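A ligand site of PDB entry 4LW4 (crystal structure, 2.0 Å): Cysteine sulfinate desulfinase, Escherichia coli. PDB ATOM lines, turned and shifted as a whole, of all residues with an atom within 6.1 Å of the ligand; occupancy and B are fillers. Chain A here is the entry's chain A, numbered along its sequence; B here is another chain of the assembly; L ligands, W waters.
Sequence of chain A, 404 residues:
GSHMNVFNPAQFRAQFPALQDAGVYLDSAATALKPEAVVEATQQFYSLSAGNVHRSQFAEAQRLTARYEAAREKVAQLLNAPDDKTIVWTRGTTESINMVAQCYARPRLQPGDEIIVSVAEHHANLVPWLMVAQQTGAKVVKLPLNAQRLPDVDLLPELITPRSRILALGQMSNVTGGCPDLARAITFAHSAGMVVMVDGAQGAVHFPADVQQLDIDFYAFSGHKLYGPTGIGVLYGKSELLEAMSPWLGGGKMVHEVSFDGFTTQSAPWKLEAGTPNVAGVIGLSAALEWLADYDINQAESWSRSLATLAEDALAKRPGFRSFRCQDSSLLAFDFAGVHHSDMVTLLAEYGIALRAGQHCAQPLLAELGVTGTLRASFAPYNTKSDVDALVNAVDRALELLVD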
ATOM      1  N   ALA A  29     -22.942 -30.940  -8.601  1.00  0.00           N
ATOM      2  CA  ALA A  29     -21.725 -30.708  -9.376  1.00  0.00           C
ATOM      3  C   ALA A  29     -21.785 -29.371 -10.140  1.00  0.00           C
ATOM      4  O   ALA A  29     -20.744 -28.818 -10.499  1.00  0.00           O
ATOM      5  CB  ALA A  29     -21.450 -31.855 -10.398  1.00  0.00           C
ATOM      6  N   ALA A  30     -22.974 -28.915 -10.446  1.00  0.00           N
ATOM      7  CA  ALA A  30     -23.177 -27.524 -10.965  1.00  0.00           C
ATOM      8  C   ALA A  30     -23.079 -26.501  -9.803  1.00  0.00           C
ATOM      9  O   ALA A  30     -22.352 -25.528  -9.878  1.00  0.00           O
ATOM     10  CB  ALA A  30     -24.530 -27.430 -11.586  1.00  0.00           C
ATOM     11  N   ARG A  91     -13.285 -14.328  -7.827  1.00  0.00           N
ATOM     12  CA  ARG A  91     -14.773 -14.504  -7.936  1.00  0.00           C
ATOM     13  C   ARG A  91     -15.150 -15.961  -8.303  1.00  0.00           C
ATOM     14  O   ARG A  91     -16.321 -16.309  -8.364  1.00  0.00           O
ATOM     15  CB  ARG A  91     -15.330 -13.459  -8.939  1.00  0.00           C
ATOM     16  CG  ARG A  91     -15.072 -13.828 -10.404  1.00  0.00           C
ATOM     17  CD  ARG A  91     -15.477 -12.699 -11.366  1.00  0.00           C
ATOM     18  NE  ARG A  91     -14.502 -11.619 -11.170  1.00  0.00           N
ATOM     19  CZ  ARG A  91     -13.684 -11.107 -12.104  1.00  0.00           C
ATOM     20  NH1 ARG A  91     -13.782 -11.513 -13.350  1.00  0.00           N
ATOM     21  NH2 ARG A  91     -12.813 -10.141 -11.804  1.00  0.00           N
ATOM     22  N   GLY A  92     -14.151 -16.806  -8.584  1.00  0.00           N
ATOM     23  CA  GLY A  92     -14.394 -18.210  -8.888  1.00  0.00           C
ATOM     24  C   GLY A  92     -13.204 -18.803  -9.612  1.00  0.00           C
ATOM     25  O   GLY A  92     -12.293 -18.098 -10.020  1.00  0.00           O
ATOM     26  N   THR A  93     -13.202 -20.103  -9.760  1.00  0.00           N
ATOM     27  CA  THR A  93     -12.202 -20.803 -10.566  1.00  0.00           C
ATOM     28  C   THR A  93     -11.905 -20.112 -11.881  1.00  0.00           C
ATOM     29  O   THR A  93     -10.743 -20.038 -12.267  1.00  0.00           O
ATOM     30  CB  THR A  93     -12.693 -22.283 -10.873  1.00  0.00           C
ATOM     31  OG1 THR A  93     -12.993 -22.910  -9.650  1.00  0.00           O
ATOM     32  CG2 THR A  93     -11.623 -23.177 -11.659  1.00  0.00           C
ATOM     33  N   THR A  94     -12.920 -19.647 -12.584  1.00  0.00           N
ATOM     34  CA  THR A  94     -12.690 -18.931 -13.823  1.00  0.00           C
ATOM     35  C   THR A  94     -11.714 -17.742 -13.719  1.00  0.00           C
ATOM     36  O   THR A  94     -10.749 -17.663 -14.475  1.00  0.00           O
ATOM     37  CB  THR A  94     -14.057 -18.576 -14.540  1.00  0.00           C
ATOM     38  OG1 THR A  94     -14.835 -19.768 -14.694  1.00  0.00           O
ATOM     39  CG2 THR A  94     -13.773 -17.989 -15.964  1.00  0.00           C
ATOM     40  N   GLU A  95     -11.948 -16.812 -12.785  1.00  0.00           N
ATOM     41  CA  GLU A  95     -11.032 -15.680 -12.671  1.00  0.00           C
ATOM     42  C   GLU A  95      -9.637 -16.232 -12.240  1.00  0.00           C
ATOM     43  O   GLU A  95      -8.626 -15.757 -12.697  1.00  0.00           O
ATOM     44  CB  GLU A  95     -11.540 -14.628 -11.643  1.00  0.00           C
ATOM     45  CG  GLU A  95     -10.626 -13.338 -11.528  1.00  0.00           C
ATOM     46  CD  GLU A  95     -11.092 -12.287 -10.540  1.00  0.00           C
ATOM     47  OE1 GLU A  95     -11.724 -12.606  -9.532  1.00  0.00           O
ATOM     48  OE2 GLU A  95     -10.777 -11.106 -10.760  1.00  0.00           O
ATOM     49  N   ILE A  97      -8.010 -18.914 -12.980  1.00  0.00           N
ATOM     50  CA  ILE A  97      -7.229 -19.418 -14.123  1.00  0.00           C
ATOM     51  C   ILE A  97      -6.795 -18.344 -15.102  1.00  0.00           C
ATOM     52  O   ILE A  97      -5.618 -18.285 -15.466  1.00  0.00           O
ATOM     53  CB  ILE A  97      -7.953 -20.605 -14.848  1.00  0.00           C
ATOM     54  CG1 ILE A  97      -8.180 -21.761 -13.825  1.00  0.00           C
ATOM     55  CG2 ILE A  97      -7.193 -20.968 -16.152  1.00  0.00           C
ATOM     56  CD1 ILE A  97      -9.121 -22.922 -14.358  1.00  0.00           C
ATOM     57  N   HIS A 122     -12.540 -28.425 -18.356  1.00  0.00           N
ATOM     58  CA  HIS A 122     -13.656 -27.516 -18.399  1.00  0.00           C
ATOM     59  C   HIS A 122     -13.165 -26.294 -19.223  1.00  0.00           C
ATOM     60  O   HIS A 122     -11.986 -25.948 -19.198  1.00  0.00           O
ATOM     61  CB  HIS A 122     -13.930 -27.105 -16.947  1.00  0.00           C
ATOM     62  CG  HIS A 122     -15.112 -26.206 -16.757  1.00  0.00           C
ATOM     63  ND1 HIS A 122     -15.109 -24.859 -17.088  1.00  0.00           N
ATOM     64  CD2 HIS A 122     -16.296 -26.438 -16.144  1.00  0.00           C
ATOM     65  CE1 HIS A 122     -16.280 -24.331 -16.766  1.00  0.00           C
ATOM     66  NE2 HIS A 122     -17.020 -25.268 -16.190  1.00  0.00           N
ATOM     67  N   ALA A 124     -13.195 -23.249 -18.558  1.00  0.00           N
ATOM     68  CA  ALA A 124     -12.394 -22.300 -17.733  1.00  0.00           C
ATOM     69  C   ALA A 124     -10.917 -22.640 -17.739  1.00  0.00           C
ATOM     70  O   ALA A 124     -10.101 -21.710 -17.527  1.00  0.00           O
ATOM     71  CB  ALA A 124     -12.855 -22.246 -16.341  1.00  0.00           C
ATOM     72  N   ASN A 125     -10.551 -23.932 -17.964  1.00  0.00           N
ATOM     73  CA  ASN A 125      -9.120 -24.306 -17.981  1.00  0.00           C
ATOM     74  C   ASN A 125      -8.665 -24.598 -19.423  1.00  0.00           C
ATOM     75  O   ASN A 125      -7.705 -25.387 -19.675  1.00  0.00           O
ATOM     76  CB  ASN A 125      -8.779 -25.486 -17.045  1.00  0.00           C
ATOM     77  CG  ASN A 125      -7.305 -25.520 -16.608  1.00  0.00           C
ATOM     78  OD1 ASN A 125      -6.770 -26.575 -16.135  1.00  0.00           O
ATOM     79  ND2 ASN A 125      -6.666 -24.380 -16.668  1.00  0.00           N
ATOM     80  N   MET A 172     -10.061 -33.125 -11.270  1.00  0.00           N
ATOM     81  CA  MET A 172     -11.226 -33.987 -11.449  1.00  0.00           C
ATOM     82  C   MET A 172     -12.219 -33.379 -12.441  1.00  0.00           C
ATOM     83  O   MET A 172     -12.610 -32.183 -12.282  1.00  0.00           O
ATOM     84  CB  MET A 172     -11.892 -34.225 -10.104  1.00  0.00           C
ATOM     85  CG  MET A 172     -13.256 -34.952 -10.141  1.00  0.00           C
ATOM     86  SD  MET A 172     -13.816 -35.056  -8.377  1.00  0.00           S
ATOM     87  CE  MET A 172     -15.340 -35.923  -8.696  1.00  0.00           C
ATOM     88  N   SER A 173     -12.648 -34.199 -13.423  1.00  0.00           N
ATOM     89  CA  SER A 173     -13.583 -33.766 -14.491  1.00  0.00           C
ATOM     90  C   SER A 173     -15.015 -33.578 -13.920  1.00  0.00           C
ATOM     91  O   SER A 173     -15.437 -34.363 -13.052  1.00  0.00           O
ATOM     92  CB  SER A 173     -13.612 -34.812 -15.628  1.00  0.00           C
ATOM     93  OG  SER A 173     -14.705 -34.580 -16.497  1.00  0.00           O
ATOM     94  N   ASN A 174     -15.716 -32.508 -14.355  1.00  0.00           N
ATOM     95  CA  ASN A 174     -17.104 -32.291 -13.946  1.00  0.00           C
ATOM     96  C   ASN A 174     -18.023 -33.148 -14.796  1.00  0.00           C
ATOM     97  O   ASN A 174     -19.215 -33.032 -14.687  1.00  0.00           O
ATOM     98  CB  ASN A 174     -17.497 -30.790 -14.110  1.00  0.00           C
ATOM     99  CG  ASN A 174     -17.346 -30.310 -15.573  1.00  0.00           C
ATOM    100  OD1 ASN A 174     -16.384 -30.626 -16.235  1.00  0.00           O
ATOM    101  ND2 ASN A 174     -18.281 -29.484 -16.025  1.00  0.00           N
ATOM    102  N   ASP A 199      -6.968 -27.308 -12.136  1.00  0.00           N
ATOM    103  CA  ASP A 199      -8.322 -26.862 -11.924  1.00  0.00           C
ATOM    104  C   ASP A 199      -8.923 -27.802 -10.820  1.00  0.00           C
ATOM    105  O   ASP A 199      -9.131 -28.985 -11.067  1.00  0.00           O
ATOM    106  CB  ASP A 199      -9.042 -26.943 -13.269  1.00  0.00           C
ATOM    107  CG  ASP A 199     -10.536 -26.670 -13.183  1.00  0.00           C
ATOM    108  OD1 ASP A 199     -11.059 -26.501 -12.066  1.00  0.00           O
ATOM    109  OD2 ASP A 199     -11.189 -26.641 -14.252  1.00  0.00           O
ATOM    110  N   GLY A 200      -9.127 -27.279  -9.613  1.00  0.00           N
ATOM    111  CA  GLY A 200      -9.626 -28.068  -8.469  1.00  0.00           C
ATOM    112  C   GLY A 200     -11.136 -27.806  -8.228  1.00  0.00           C
ATOM    113  O   GLY A 200     -11.671 -28.155  -7.196  1.00  0.00           O
ATOM    114  N   ALA A 201     -11.838 -27.224  -9.182  1.00  0.00           N
ATOM    115  CA  ALA A 201     -13.261 -26.836  -8.894  1.00  0.00           C
ATOM    116  C   ALA A 201     -14.103 -28.047  -8.416  1.00  0.00           C
ATOM    117  O   ALA A 201     -14.912 -27.927  -7.482  1.00  0.00           O
ATOM    118  CB  ALA A 201     -13.924 -26.206 -10.186  1.00  0.00           C
ATOM    119  N   GLN A 202     -13.940 -29.211  -9.062  1.00  0.00           N
ATOM    120  CA  GLN A 202     -14.531 -30.433  -8.486  1.00  0.00           C
ATOM    121  C   GLN A 202     -13.681 -31.097  -7.447  1.00  0.00           C
ATOM    122  O   GLN A 202     -14.216 -31.635  -6.496  1.00  0.00           O
ATOM    123  CB  GLN A 202     -14.878 -31.496  -9.564  1.00  0.00           C
ATOM    124  CG  GLN A 202     -15.892 -30.989 -10.629  1.00  0.00           C
ATOM    125  CD  GLN A 202     -17.286 -30.768 -10.068  1.00  0.00           C
ATOM    126  OE1 GLN A 202     -17.745 -31.465  -9.133  1.00  0.00           O
ATOM    127  NE2 GLN A 202     -17.969 -29.777 -10.636  1.00  0.00           N
ATOM    128  N   SER A 222     -13.945 -22.999  -6.631  1.00  0.00           N
ATOM    129  CA  SER A 222     -15.052 -22.032  -6.418  1.00  0.00           C
ATOM    130  C   SER A 222     -15.793 -22.337  -5.139  1.00  0.00           C
ATOM    131  O   SER A 222     -16.142 -23.505  -4.853  1.00  0.00           O
ATOM    132  CB  SER A 222     -16.067 -22.065  -7.573  1.00  0.00           C
ATOM    133  OG  SER A 222     -15.482 -21.863  -8.880  1.00  0.00           O
ATOM    134  N   HIS A 224     -18.981 -21.776  -4.538  1.00  0.00           N
ATOM    135  CA  HIS A 224     -20.435 -22.138  -4.631  1.00  0.00           C
ATOM    136  C   HIS A 224     -20.608 -23.667  -4.732  1.00  0.00           C
ATOM    137  O   HIS A 224     -21.648 -24.244  -4.326  1.00  0.00           O
ATOM    138  CB  HIS A 224     -21.166 -21.388  -5.757  1.00  0.00           C
ATOM    139  CG  HIS A 224     -20.713 -21.778  -7.160  1.00  0.00           C
ATOM    140  ND1 HIS A 224     -21.360 -22.733  -7.920  1.00  0.00           N
ATOM    141  CD2 HIS A 224     -19.666 -21.325  -7.905  1.00  0.00           C
ATOM    142  CE1 HIS A 224     -20.743 -22.843  -9.095  1.00  0.00           C
ATOM    143  NE2 HIS A 224     -19.684 -22.017  -9.086  1.00  0.00           N
ATOM    144  N   LYS A 225     -19.556 -24.348  -5.237  1.00  0.00           N
ATOM    145  CA  LYS A 225     -19.556 -25.813  -5.326  1.00  0.00           C
ATOM    146  C   LYS A 225     -19.152 -26.472  -4.022  1.00  0.00           C
ATOM    147  O   LYS A 225     -19.522 -27.621  -3.766  1.00  0.00           O
ATOM    148  CB  LYS A 225     -18.646 -26.324  -6.468  1.00  0.00           C
ATOM    149  CG  LYS A 225     -19.251 -25.923  -7.811  1.00  0.00           C
ATOM    150  CD  LYS A 225     -18.332 -26.230  -8.977  1.00  0.00           C
ATOM    151  CE  LYS A 225     -19.205 -26.101 -10.198  1.00  0.00           C
ATOM    152  NZ  LYS A 225     -18.280 -26.143 -11.347  1.00  0.00           N
ATOM    153  N   ARG A 376     -26.477 -35.572 -16.344  1.00  0.00           N
ATOM    154  CA  ARG A 376     -25.528 -35.834 -15.273  1.00  0.00           C
ATOM    155  C   ARG A 376     -26.253 -35.737 -13.939  1.00  0.00           C
ATOM    156  O   ARG A 376     -26.889 -34.748 -13.673  1.00  0.00           O
ATOM    157  CB  ARG A 376     -24.324 -34.855 -15.351  1.00  0.00           C
ATOM    158  CG  ARG A 376     -23.195 -35.082 -14.227  1.00  0.00           C
ATOM    159  CD  ARG A 376     -22.309 -33.850 -14.077  1.00  0.00           C
ATOM    160  NE  ARG A 376     -23.033 -32.654 -13.636  1.00  0.00           N
ATOM    161  CZ  ARG A 376     -22.595 -31.394 -13.761  1.00  0.00           C
ATOM    162  NH1 ARG A 376     -21.410 -31.135 -14.263  1.00  0.00           N
ATOM    163  NH2 ARG A 376     -23.358 -30.355 -13.367  1.00  0.00           N
ATOM    164  N   ALA B 274     -17.651 -14.253 -18.089  1.00  0.00           N
ATOM    165  CA  ALA B 274     -17.205 -15.642 -18.067  1.00  0.00           C
ATOM    166  C   ALA B 274     -17.612 -16.309 -16.737  1.00  0.00           C
ATOM    167  O   ALA B 274     -17.485 -15.681 -15.687  1.00  0.00           O
ATOM    168  CB  ALA B 274     -15.601 -15.697 -18.210  1.00  0.00           C
ATOM    169  N   GLY B 275     -17.925 -17.594 -16.788  1.00  0.00           N
ATOM    170  CA  GLY B 275     -18.054 -18.416 -15.628  1.00  0.00           C
ATOM    171  C   GLY B 275     -19.364 -18.205 -14.850  1.00  0.00           C
ATOM    172  O   GLY B 275     -20.281 -17.431 -15.280  1.00  0.00           O
ATOM    173  N   THR B 276     -19.489 -18.913 -13.754  1.00  0.00           N
ATOM    174  CA  THR B 276     -20.686 -18.762 -12.892  1.00  0.00           C
ATOM    175  C   THR B 276     -20.805 -17.311 -12.332  1.00  0.00           C
ATOM    176  O   THR B 276     -19.839 -16.809 -11.683  1.00  0.00           O
ATOM    177  CB  THR B 276     -20.657 -19.784 -11.712  1.00  0.00           C
ATOM    178  OG1 THR B 276     -20.520 -21.112 -12.260  1.00  0.00           O
ATOM    179  CG2 THR B 276     -21.945 -19.686 -10.852  1.00  0.00           C
ATOM    180  N   PRO B 277     -21.943 -16.626 -12.606  1.00  0.00           N
ATOM    181  CA  PRO B 277     -22.188 -15.285 -12.078  1.00  0.00           C
ATOM    182  C   PRO B 277     -22.226 -15.313 -10.551  1.00  0.00           C
ATOM    183  O   PRO B 277     -22.472 -16.380  -9.940  1.00  0.00           O
ATOM    184  CB  PRO B 277     -23.647 -14.957 -12.556  1.00  0.00           C
ATOM    185  CG  PRO B 277     -23.884 -15.708 -13.746  1.00  0.00           C
ATOM    186  CD  PRO B 277     -23.083 -17.087 -13.431  1.00  0.00           C
HETATM  187  N1  LIG L   1     -13.666 -26.248 -13.669  1.00  0.00           N
HETATM  188  C1  LIG L   1     -14.478 -27.303 -13.310  1.00  0.00           C
HETATM  189  C2  LIG L   1     -13.948 -28.638 -13.393  1.00  0.00           C
HETATM  190  C3  LIG L   1     -15.791 -26.978 -12.907  1.00  0.00           C
HETATM  191  O1  LIG L   1     -16.708 -27.921 -12.505  1.00  0.00           O
HETATM  192  C4  LIG L   1     -16.189 -25.631 -12.832  1.00  0.00           C
HETATM  193  C5  LIG L   1     -17.485 -25.279 -12.422  1.00  0.00           C
HETATM  194  C6  LIG L   1     -15.343 -24.588 -13.201  1.00  0.00           C
HETATM  195  C7  LIG L   1     -14.080 -24.928 -13.646  1.00  0.00           C
HETATM  196  C8  LIG L   1     -15.803 -23.207 -13.242  1.00  0.00           C
HETATM  197  O2  LIG L   1     -16.080 -22.534 -11.953  1.00  0.00           O
HETATM  198  P1  LIG L   1     -16.841 -21.157 -11.888  1.00  0.00           P
HETATM  199  O3  LIG L   1     -17.890 -21.043 -12.929  1.00  0.00           O
HETATM  200  O4  LIG L   1     -15.827 -20.097 -12.256  1.00  0.00           O
HETATM  201  O5  LIG L   1     -17.201 -21.047 -10.459  1.00  0.00           O
HETATM  202  O   HOH W   1     -18.388 -21.806 -15.540  1.00  0.00           O
HETATM  203  O   HOH W   2     -17.739 -18.657  -8.911  1.00  0.00           O
HETATM  204  O   HOH W   3     -19.476 -24.932 -14.912  1.00  0.00           O
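NZ of Lys 225 is bonded to C5 of the ligand. OD2 of Asp 199 lies within hydrogen-bond range of N1 of the ligand (2.6 Å). NE2 of Gln 202 sits at hydrogen-bond distance from O1 of the ligand. The side-chain hydroxyl (OG1) of Thr 94 lies within hydrogen-bond range of an oxygen (O4) of the ligand (2.7 Å). An oxygen (O3) of the ligand sits at hydrogen-bond distance from the backbone NH of Thr 276 of chain B, 2.8 Å away. An oxygen (O3) of the ligand is in hydrogen-bond range of the side-chain hydroxyl of Thr 276 of chain B (2.7 Å). OG of Ser 222 is in hydrogen-bond range of O5 of the ligand. The backbone NH (N) of Thr 94 is in hydrogen-bond range of an oxygen (O4) of the ligand, 3.0 Å away. NE2 of His 224 is in hydrogen-bond range of O5 of the ligand (3.0 Å).
The side-chain carboxylate (OD1) of Asp 199 lies within hydrogen-bond range of the backbone NH (N) of Ala 201, at 3.1 Å. The guanidinium group (NH1) of Arg 376 is in hydrogen-bond range of the backbone carbonyl oxygen (O) of Asn 174, at 2.9 Å. The backbone NH of Ala 124 is in hydrogen-bond range of a ring nitrogen (ND1) of His 122 (2.9 Å). The side-chain hydroxyl (OG) of Ser 222 lies within hydrogen-bond range of the side-chain hydroxyl (OG1) of Thr 93. The side-chain hydroxyl (OG1) of Thr 276 of chain B lies within hydrogen-bond range of a ring nitrogen (NE2) of His 224. The side-chain amide nitrogen (NE2) of Gln 202 sits at hydrogen-bond distance from the backbone carbonyl oxygen (O) of Ala 29, at 2.9 Å.
Merely in contact with the ligand: Gly 92 (3.9 Å), Thr 93 (3.6 Å), His 122 (3.3 Å), Ala 124 (3.99 Å), Met 172 (3.9 Å), Asn 174 (3.4 Å), Ala 201 (3.4 Å) and Gly 275 of chain B (3.7 Å). Hydrophobic or aromatic side chains within 4 Å of the ligand: His 122, Ala 124, Ala 201 and His 224. 15 residues have an atom within 4 Å of the ligand: Gly 92, Thr 93, Thr 94, His 122, Ala 124, Met 172, Asn 174, Asp 199, Ala 201, Gln 202, Ser 222, His 224, Lys 225, Gly 275 of chain B and Thr 276 of chain B.
Water W2 bridges the backbone carbonyl oxygen of Arg 91 (2.8 Å) and an oxygen (O5) of the ligand (2.9 Å).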
